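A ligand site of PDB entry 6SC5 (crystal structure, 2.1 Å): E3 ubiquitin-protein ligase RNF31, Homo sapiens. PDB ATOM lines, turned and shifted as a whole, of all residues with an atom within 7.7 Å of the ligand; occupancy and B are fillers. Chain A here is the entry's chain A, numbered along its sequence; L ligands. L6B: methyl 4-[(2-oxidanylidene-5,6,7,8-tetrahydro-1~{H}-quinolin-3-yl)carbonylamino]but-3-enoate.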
ATOM      1  N   ILE A 173      -5.686  28.443  -6.153  1.00  0.00           N
ATOM      2  CA  ILE A 173      -6.297  27.381  -6.952  1.00  0.00           C
ATOM      3  C   ILE A 173      -7.015  26.433  -6.008  1.00  0.00           C
ATOM      4  O   ILE A 173      -6.386  25.767  -5.181  1.00  0.00           O
ATOM      5  CB  ILE A 173      -5.248  26.646  -7.790  1.00  0.00           C
ATOM      6  CG1 ILE A 173      -4.516  27.621  -8.728  1.00  0.00           C
ATOM      7  CG2 ILE A 173      -5.891  25.511  -8.579  1.00  0.00           C
ATOM      8  CD1 ILE A 173      -3.373  26.989  -9.493  1.00  0.00           C
ATOM      9  N   PHE A 180      -9.357  21.330  -1.708  1.00  0.00           N
ATOM     10  CA  PHE A 180      -8.050  21.719  -1.194  1.00  0.00           C
ATOM     11  C   PHE A 180      -7.569  22.970  -1.911  1.00  0.00           C
ATOM     12  O   PHE A 180      -7.581  23.040  -3.147  1.00  0.00           O
ATOM     13  CB  PHE A 180      -7.040  20.576  -1.378  1.00  0.00           C
ATOM     14  CG  PHE A 180      -5.780  20.731  -0.570  1.00  0.00           C
ATOM     15  CD1 PHE A 180      -4.765  21.575  -0.996  1.00  0.00           C
ATOM     16  CD2 PHE A 180      -5.605  20.015   0.606  1.00  0.00           C
ATOM     17  CE1 PHE A 180      -3.602  21.712  -0.255  1.00  0.00           C
ATOM     18  CE2 PHE A 180      -4.444  20.143   1.348  1.00  0.00           C
ATOM     19  CZ  PHE A 180      -3.443  20.991   0.917  1.00  0.00           C
ATOM     20  N   TYR A 182      -4.746  25.804  -2.946  1.00  0.00           N
ATOM     21  CA  TYR A 182      -3.329  26.022  -3.188  1.00  0.00           C
ATOM     22  C   TYR A 182      -3.097  27.506  -3.434  1.00  0.00           C
ATOM     23  O   TYR A 182      -3.721  28.091  -4.334  1.00  0.00           O
ATOM     24  CB  TYR A 182      -2.837  25.200  -4.392  1.00  0.00           C
ATOM     25  CG  TYR A 182      -3.106  23.716  -4.295  1.00  0.00           C
ATOM     26  CD1 TYR A 182      -4.310  23.185  -4.733  1.00  0.00           C
ATOM     27  CD2 TYR A 182      -2.153  22.848  -3.785  1.00  0.00           C
ATOM     28  CE1 TYR A 182      -4.568  21.822  -4.655  1.00  0.00           C
ATOM     29  CE2 TYR A 182      -2.396  21.491  -3.703  1.00  0.00           C
ATOM     30  CZ  TYR A 182      -3.602  20.983  -4.138  1.00  0.00           C
ATOM     31  OH  TYR A 182      -3.842  19.635  -4.057  1.00  0.00           O
ATOM     32  N   LEU A 184      -1.157  29.461  -5.099  1.00  0.00           N
ATOM     33  CA  LEU A 184      -0.210  29.452  -6.197  1.00  0.00           C
ATOM     34  C   LEU A 184      -0.786  30.186  -7.397  1.00  0.00           C
ATOM     35  O   LEU A 184      -2.005  30.238  -7.593  1.00  0.00           O
ATOM     36  CB  LEU A 184       0.155  28.030  -6.619  1.00  0.00           C
ATOM     37  CG  LEU A 184       0.557  27.060  -5.509  1.00  0.00           C
ATOM     38  CD1 LEU A 184       0.544  25.632  -6.033  1.00  0.00           C
ATOM     39  CD2 LEU A 184       1.911  27.426  -4.952  1.00  0.00           C
ATOM     40  N   ALA A 185       0.109  30.753  -8.204  1.00  0.00           N
ATOM     41  CA  ALA A 185      -0.273  31.271  -9.495  1.00  0.00           C
ATOM     42  C   ALA A 185      -0.369  30.136 -10.503  1.00  0.00           C
ATOM     43  O   ALA A 185       0.175  29.045 -10.315  1.00  0.00           O
ATOM     44  CB  ALA A 185       0.729  32.326  -9.979  1.00  0.00           C
ATOM     45  N   ARG A 186      -1.098  30.390 -11.596  1.00  0.00           N
ATOM     46  CA  ARG A 186      -1.298  29.371 -12.615  1.00  0.00           C
ATOM     47  C   ARG A 186      -0.159  29.329 -13.628  1.00  0.00           C
ATOM     48  O   ARG A 186       0.235  28.253 -14.075  1.00  0.00           O
ATOM     49  CB  ARG A 186      -2.624  29.602 -13.335  1.00  0.00           C
ATOM     50  CG  ARG A 186      -3.843  29.439 -12.431  1.00  0.00           C
ATOM     51  CD  ARG A 186      -4.889  30.503 -12.699  1.00  0.00           C
ATOM     52  NE  ARG A 186      -6.158  30.175 -12.069  1.00  0.00           N
ATOM     53  CZ  ARG A 186      -6.438  30.359 -10.781  1.00  0.00           C
ATOM     54  NH1 ARG A 186      -7.628  30.026 -10.298  1.00  0.00           N
ATOM     55  NH2 ARG A 186      -5.513  30.881  -9.973  1.00  0.00           N
ATOM     56  N   GLY A 187       0.395  30.492 -13.987  1.00  0.00           N
ATOM     57  CA  GLY A 187       1.470  30.505 -14.956  1.00  0.00           C
ATOM     58  C   GLY A 187       0.961  30.224 -16.360  1.00  0.00           C
ATOM     59  O   GLY A 187      -0.081  30.727 -16.786  1.00  0.00           O
ATOM     60  N   GLY A 188       1.704  29.395 -17.085  1.00  0.00           N
ATOM     61  CA  GLY A 188       1.345  29.058 -18.451  1.00  0.00           C
ATOM     62  C   GLY A 188       0.769  27.671 -18.603  1.00  0.00           C
ATOM     63  O   GLY A 188       0.229  27.332 -19.666  1.00  0.00           O
ATOM     64  N   CYS A 189       0.864  26.865 -17.550  1.00  0.00           N
ATOM     65  CA  CYS A 189       0.359  25.498 -17.569  1.00  0.00           C
ATOM     66  C   CYS A 189      -1.018  25.461 -16.893  1.00  0.00           C
ATOM     67  O   CYS A 189      -1.145  25.807 -15.721  1.00  0.00           O
ATOM     68  CB  CYS A 189       1.326  24.549 -16.849  1.00  0.00           C
ATOM     69  SG  CYS A 189       0.870  22.804 -16.925  1.00  0.00           S
ATOM     70  N   MET A 190      -2.033  25.044 -17.653  1.00  0.00           N
ATOM     71  CA  MET A 190      -3.391  24.988 -17.141  1.00  0.00           C
ATOM     72  C   MET A 190      -3.767  23.641 -16.545  1.00  0.00           C
ATOM     73  O   MET A 190      -4.672  23.573 -15.713  1.00  0.00           O
ATOM     74  CB  MET A 190      -4.392  25.348 -18.246  1.00  0.00           C
ATOM     75  CG  MET A 190      -4.041  26.592 -19.035  1.00  0.00           C
ATOM     76  SD  MET A 190      -3.894  28.061 -17.997  1.00  0.00           S
ATOM     77  CE  MET A 190      -5.500  28.052 -17.213  1.00  0.00           C
ATOM     78  N   HIS A 191      -3.093  22.563 -16.967  1.00  0.00           N
ATOM     79  CA  HIS A 191      -3.419  21.209 -16.526  1.00  0.00           C
ATOM     80  C   HIS A 191      -2.915  21.021 -15.105  1.00  0.00           C
ATOM     81  O   HIS A 191      -1.724  20.781 -14.875  1.00  0.00           O
ATOM     82  CB  HIS A 191      -2.805  20.191 -17.479  1.00  0.00           C
ATOM     83  CG  HIS A 191      -3.197  18.772 -17.178  1.00  0.00           C
ATOM     84  ND1 HIS A 191      -2.697  17.705 -17.894  1.00  0.00           N
ATOM     85  CD2 HIS A 191      -4.027  18.248 -16.243  1.00  0.00           C
ATOM     86  CE1 HIS A 191      -3.210  16.581 -17.408  1.00  0.00           C
ATOM     87  NE2 HIS A 191      -4.019  16.886 -16.410  1.00  0.00           N
ATOM     88  N   PHE A 192      -3.816  21.132 -14.131  1.00  0.00           N
ATOM     89  CA  PHE A 192      -3.469  21.012 -12.722  1.00  0.00           C
ATOM     90  C   PHE A 192      -3.696  19.590 -12.221  1.00  0.00           C
ATOM     91  O   PHE A 192      -4.659  18.934 -12.623  1.00  0.00           O
ATOM     92  CB  PHE A 192      -4.285  22.001 -11.876  1.00  0.00           C
ATOM     93  CG  PHE A 192      -3.676  22.278 -10.529  1.00  0.00           C
ATOM     94  CD1 PHE A 192      -3.992  21.500  -9.429  1.00  0.00           C
ATOM     95  CD2 PHE A 192      -2.763  23.318 -10.367  1.00  0.00           C
ATOM     96  CE1 PHE A 192      -3.434  21.752  -8.193  1.00  0.00           C
ATOM     97  CE2 PHE A 192      -2.202  23.580  -9.131  1.00  0.00           C
ATOM     98  CZ  PHE A 192      -2.537  22.797  -8.044  1.00  0.00           C
ATOM     99  N   HIS A 193      -2.805  19.140 -11.347  1.00  0.00           N
ATOM    100  CA  HIS A 193      -2.907  17.849 -10.686  1.00  0.00           C
ATOM    101  C   HIS A 193      -2.988  18.082  -9.189  1.00  0.00           C
ATOM    102  O   HIS A 193      -2.091  18.699  -8.605  1.00  0.00           O
ATOM    103  CB  HIS A 193      -1.701  16.959 -11.011  1.00  0.00           C
ATOM    104  CG  HIS A 193      -1.642  16.498 -12.434  1.00  0.00           C
ATOM    105  ND1 HIS A 193      -1.091  17.261 -13.445  1.00  0.00           N
ATOM    106  CD2 HIS A 193      -2.052  15.338 -13.012  1.00  0.00           C
ATOM    107  CE1 HIS A 193      -1.177  16.595 -14.583  1.00  0.00           C
ATOM    108  NE2 HIS A 193      -1.746  15.426 -14.350  1.00  0.00           N
ATOM    109  N   CYS A 194      -4.067  17.610  -8.567  1.00  0.00           N
ATOM    110  CA  CYS A 194      -4.256  17.746  -7.127  1.00  0.00           C
ATOM    111  C   CYS A 194      -3.599  16.567  -6.422  1.00  0.00           C
ATOM    112  O   CYS A 194      -3.935  15.408  -6.704  1.00  0.00           O
ATOM    113  CB  CYS A 194      -5.730  17.839  -6.773  1.00  0.00           C
ATOM    114  SG  CYS A 194      -6.056  18.024  -5.001  1.00  0.00           S
ATOM    115  N   THR A 195      -2.680  16.858  -5.504  1.00  0.00           N
ATOM    116  CA  THR A 195      -1.967  15.799  -4.796  1.00  0.00           C
ATOM    117  C   THR A 195      -2.879  15.028  -3.850  1.00  0.00           C
ATOM    118  O   THR A 195      -2.692  13.829  -3.647  1.00  0.00           O
ATOM    119  CB  THR A 195      -0.776  16.371  -4.029  1.00  0.00           C
ATOM    120  OG1 THR A 195      -1.160  17.632  -3.454  1.00  0.00           O
ATOM    121  CG2 THR A 195       0.403  16.586  -4.956  1.00  0.00           C
ATOM    122  N   GLN A 196      -3.856  15.709  -3.259  1.00  0.00           N
ATOM    123  CA  GLN A 196      -4.721  15.062  -2.283  1.00  0.00           C
ATOM    124  C   GLN A 196      -5.725  14.136  -2.937  1.00  0.00           C
ATOM    125  O   GLN A 196      -6.000  13.046  -2.415  1.00  0.00           O
ATOM    126  CB  GLN A 196      -5.444  16.106  -1.433  1.00  0.00           C
ATOM    127  N   HIS A 199      -7.427  14.379  -8.788  1.00  0.00           N
ATOM    128  CA  HIS A 199      -8.270  14.903  -9.855  1.00  0.00           C
ATOM    129  C   HIS A 199      -7.476  15.876 -10.712  1.00  0.00           C
ATOM    130  O   HIS A 199      -6.695  16.681 -10.216  1.00  0.00           O
ATOM    131  CB  HIS A 199      -9.499  15.600  -9.268  1.00  0.00           C
ATOM    132  CG  HIS A 199     -10.455  16.111 -10.295  1.00  0.00           C
ATOM    133  ND1 HIS A 199     -10.822  17.440 -10.363  1.00  0.00           N
ATOM    134  CD2 HIS A 199     -11.125  15.482 -11.294  1.00  0.00           C
ATOM    135  CE1 HIS A 199     -11.676  17.605 -11.360  1.00  0.00           C
ATOM    136  NE2 HIS A 199     -11.879  16.433 -11.935  1.00  0.00           N
ATOM    137  N   GLN A 200      -7.678  15.779 -12.025  1.00  0.00           N
ATOM    138  CA  GLN A 200      -7.009  16.624 -12.997  1.00  0.00           C
ATOM    139  C   GLN A 200      -8.026  17.612 -13.559  1.00  0.00           C
ATOM    140  O   GLN A 200      -9.074  17.195 -14.072  1.00  0.00           O
ATOM    141  CB  GLN A 200      -6.389  15.790 -14.118  1.00  0.00           C
ATOM    142  CG  GLN A 200      -5.470  14.692 -13.606  1.00  0.00           C
ATOM    143  CD  GLN A 200      -4.838  13.896 -14.730  1.00  0.00           C
ATOM    144  OE1 GLN A 200      -4.706  14.382 -15.852  1.00  0.00           O
ATOM    145  NE2 GLN A 200      -4.445  12.661 -14.437  1.00  0.00           N
ATOM    146  N   PHE A 201      -7.705  18.896 -13.472  1.00  0.00           N
ATOM    147  CA  PHE A 201      -8.634  19.942 -13.894  1.00  0.00           C
ATOM    148  C   PHE A 201      -7.844  21.122 -14.427  1.00  0.00           C
ATOM    149  O   PHE A 201      -6.623  21.226 -14.244  1.00  0.00           O
ATOM    150  CB  PHE A 201      -9.544  20.375 -12.742  1.00  0.00           C
ATOM    151  CG  PHE A 201      -8.807  20.955 -11.568  1.00  0.00           C
ATOM    152  CD1 PHE A 201      -8.234  20.140 -10.603  1.00  0.00           C
ATOM    153  CD2 PHE A 201      -8.673  22.333 -11.433  1.00  0.00           C
ATOM    154  CE1 PHE A 201      -7.552  20.666  -9.528  1.00  0.00           C
ATOM    155  CE2 PHE A 201      -7.997  22.872 -10.354  1.00  0.00           C
ATOM    156  CZ  PHE A 201      -7.426  22.035  -9.402  1.00  0.00           C
ATOM    157  N   SER A 203      -6.804  24.884 -14.186  1.00  0.00           N
ATOM    158  CA  SER A 203      -6.712  25.887 -13.140  1.00  0.00           C
ATOM    159  C   SER A 203      -7.393  27.196 -13.506  1.00  0.00           C
ATOM    160  O   SER A 203      -7.579  28.042 -12.628  1.00  0.00           O
ATOM    161  CB  SER A 203      -5.247  26.150 -12.784  1.00  0.00           C
ATOM    162  OG  SER A 203      -4.486  26.425 -13.944  1.00  0.00           O
ATOM    163  N   GLU A 277       6.816  29.515  -7.478  1.00  0.00           N
ATOM    164  CA  GLU A 277       6.353  28.249  -8.016  1.00  0.00           C
ATOM    165  C   GLU A 277       6.861  27.110  -7.142  1.00  0.00           C
ATOM    166  O   GLU A 277       7.727  27.297  -6.283  1.00  0.00           O
ATOM    167  CB  GLU A 277       6.814  28.069  -9.464  1.00  0.00           C
ATOM    168  CG  GLU A 277       6.351  29.167 -10.406  1.00  0.00           C
ATOM    169  CD  GLU A 277       6.665  28.875 -11.860  1.00  0.00           C
ATOM    170  OE1 GLU A 277       5.888  29.299 -12.743  1.00  0.00           O
ATOM    171  OE2 GLU A 277       7.696  28.225 -12.121  1.00  0.00           O
ATOM    172  N   GLN A 278       6.310  25.929  -7.369  1.00  0.00           N
ATOM    173  CA  GLN A 278       6.626  24.749  -6.574  1.00  0.00           C
ATOM    174  C   GLN A 278       7.393  23.753  -7.442  1.00  0.00           C
ATOM    175  O   GLN A 278       6.810  23.117  -8.327  1.00  0.00           O
ATOM    176  CB  GLN A 278       5.361  24.111  -5.998  1.00  0.00           C
ATOM    177  CG  GLN A 278       4.535  25.051  -5.140  1.00  0.00           C
ATOM    178  CD  GLN A 278       4.521  24.639  -3.682  1.00  0.00           C
ATOM    179  OE1 GLN A 278       3.883  23.640  -3.307  1.00  0.00           O
ATOM    180  NE2 GLN A 278       5.205  25.397  -2.846  1.00  0.00           N
ATOM    181  N   LYS A 279       8.687  23.621  -7.175  1.00  0.00           N
ATOM    182  CA  LYS A 279       9.533  22.647  -7.846  1.00  0.00           C
ATOM    183  C   LYS A 279       9.597  21.371  -7.018  1.00  0.00           C
ATOM    184  O   LYS A 279       9.879  21.423  -5.821  1.00  0.00           O
ATOM    185  CB  LYS A 279      10.939  23.207  -8.073  1.00  0.00           C
ATOM    186  N   LEU A 285       8.552  19.570  -1.852  1.00  0.00           N
ATOM    187  CA  LEU A 285       8.282  20.708  -2.715  1.00  0.00           C
ATOM    188  C   LEU A 285       9.090  21.903  -2.230  1.00  0.00           C
ATOM    189  O   LEU A 285       9.081  22.225  -1.037  1.00  0.00           O
ATOM    190  CB  LEU A 285       6.787  21.041  -2.723  1.00  0.00           C
ATOM    191  CG  LEU A 285       5.877  20.010  -3.393  1.00  0.00           C
ATOM    192  CD1 LEU A 285       4.424  20.450  -3.347  1.00  0.00           C
ATOM    193  CD2 LEU A 285       6.319  19.753  -4.826  1.00  0.00           C
HETATM  194  C01 L6B L   1       1.984  22.520  -6.924  1.00  0.00           C
HETATM  195  C02 L6B L   1       1.417  21.890  -5.633  1.00  0.00           C
HETATM  196  C03 L6B L   1       1.326  20.364  -5.741  1.00  0.00           C
HETATM  197  C04 L6B L   1       0.483  19.910  -6.936  1.00  0.00           C
HETATM  198  C05 L6B L   1       0.622  20.793  -8.191  1.00  0.00           C
HETATM  199  C06 L6B L   1       1.297  21.970  -8.186  1.00  0.00           C
HETATM  200  C08 L6B L   1       0.090  21.015 -10.468  1.00  0.00           C
HETATM  201  C09 L6B L   1       0.774  22.224 -10.542  1.00  0.00           C
HETATM  202  C10 L6B L   1       1.389  22.724  -9.394  1.00  0.00           C
HETATM  203  C11 L6B L   1       0.826  23.004 -11.852  1.00  0.00           C
HETATM  204  C13 L6B L   1       0.256  23.235 -14.288  1.00  0.00           C
HETATM  205  C14 L6B L   1       1.305  22.639 -15.227  1.00  0.00           C
HETATM  206  C15 L6B L   1       2.724  22.946 -14.759  1.00  0.00           C
HETATM  207  C16 L6B L   1       3.761  22.060 -15.436  1.00  0.00           C
HETATM  208  C18 L6B L   1       4.694  22.519 -17.535  1.00  0.00           C
HETATM  209  N07 L6B L   1       0.026  20.340  -9.334  1.00  0.00           N
HETATM  210  N12 L6B L   1       0.192  22.484 -13.048  1.00  0.00           N
HETATM  211  O17 L6B L   1       4.820  22.635 -16.152  1.00  0.00           O
HETATM  212  O19 L6B L   1      -0.535  20.498 -11.602  1.00  0.00           O
HETATM  213  O20 L6B L   1       1.394  24.042 -11.895  1.00  0.00           O
HETATM  214  O21 L6B L   1       3.666  20.877 -15.345  1.00  0.00           O
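A nitrogen (N12) of the ligand lies within hydrogen-bond range of the backbone carbonyl oxygen of His 191, 3.1 Å away.
A nitrogen (N07) of the ligand lies within hydrogen-bond range of the backbone carbonyl oxygen (O) of His 193, 2.8 Å away.
SG of Cys 189 is covalently linked to C14 of the ligand, at 1.8 Å.
The backbone NH (N) of His 193 lies within hydrogen-bond range of an oxygen (O19) of the ligand (2.7 Å).
Merely in contact with the ligand: Leu 184 (3.5 Å), Phe 192 (3.2 Å), Thr 195 (3.9 Å), Gln 278 (3.8 Å) and Leu 285 (3.9 Å).
Of the 24 residues printed, 8 come within 4 Å of the ligand.
The nearest printed residue that does not touch the ligand is Tyr 182 (4.1 Å).
N of Phe 192 sits at hydrogen-bond distance from O of Phe 201, 2.8 Å away.
NE2 of His 191 is in hydrogen-bond range of OE1 of Gln 200 (2.7 Å).
A ring nitrogen (NE2) of His 193 lies close to the side-chain amide oxygen (OE1) of Gln 200 (3.5 Å).
The side-chain hydroxyl (OH) of Tyr 182 lies within hydrogen-bond range of the backbone NH (N) of Thr 195 (3.3 Å).
NE2 of His 191 lies close to NE2 of His 193, at 3.4 Å.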
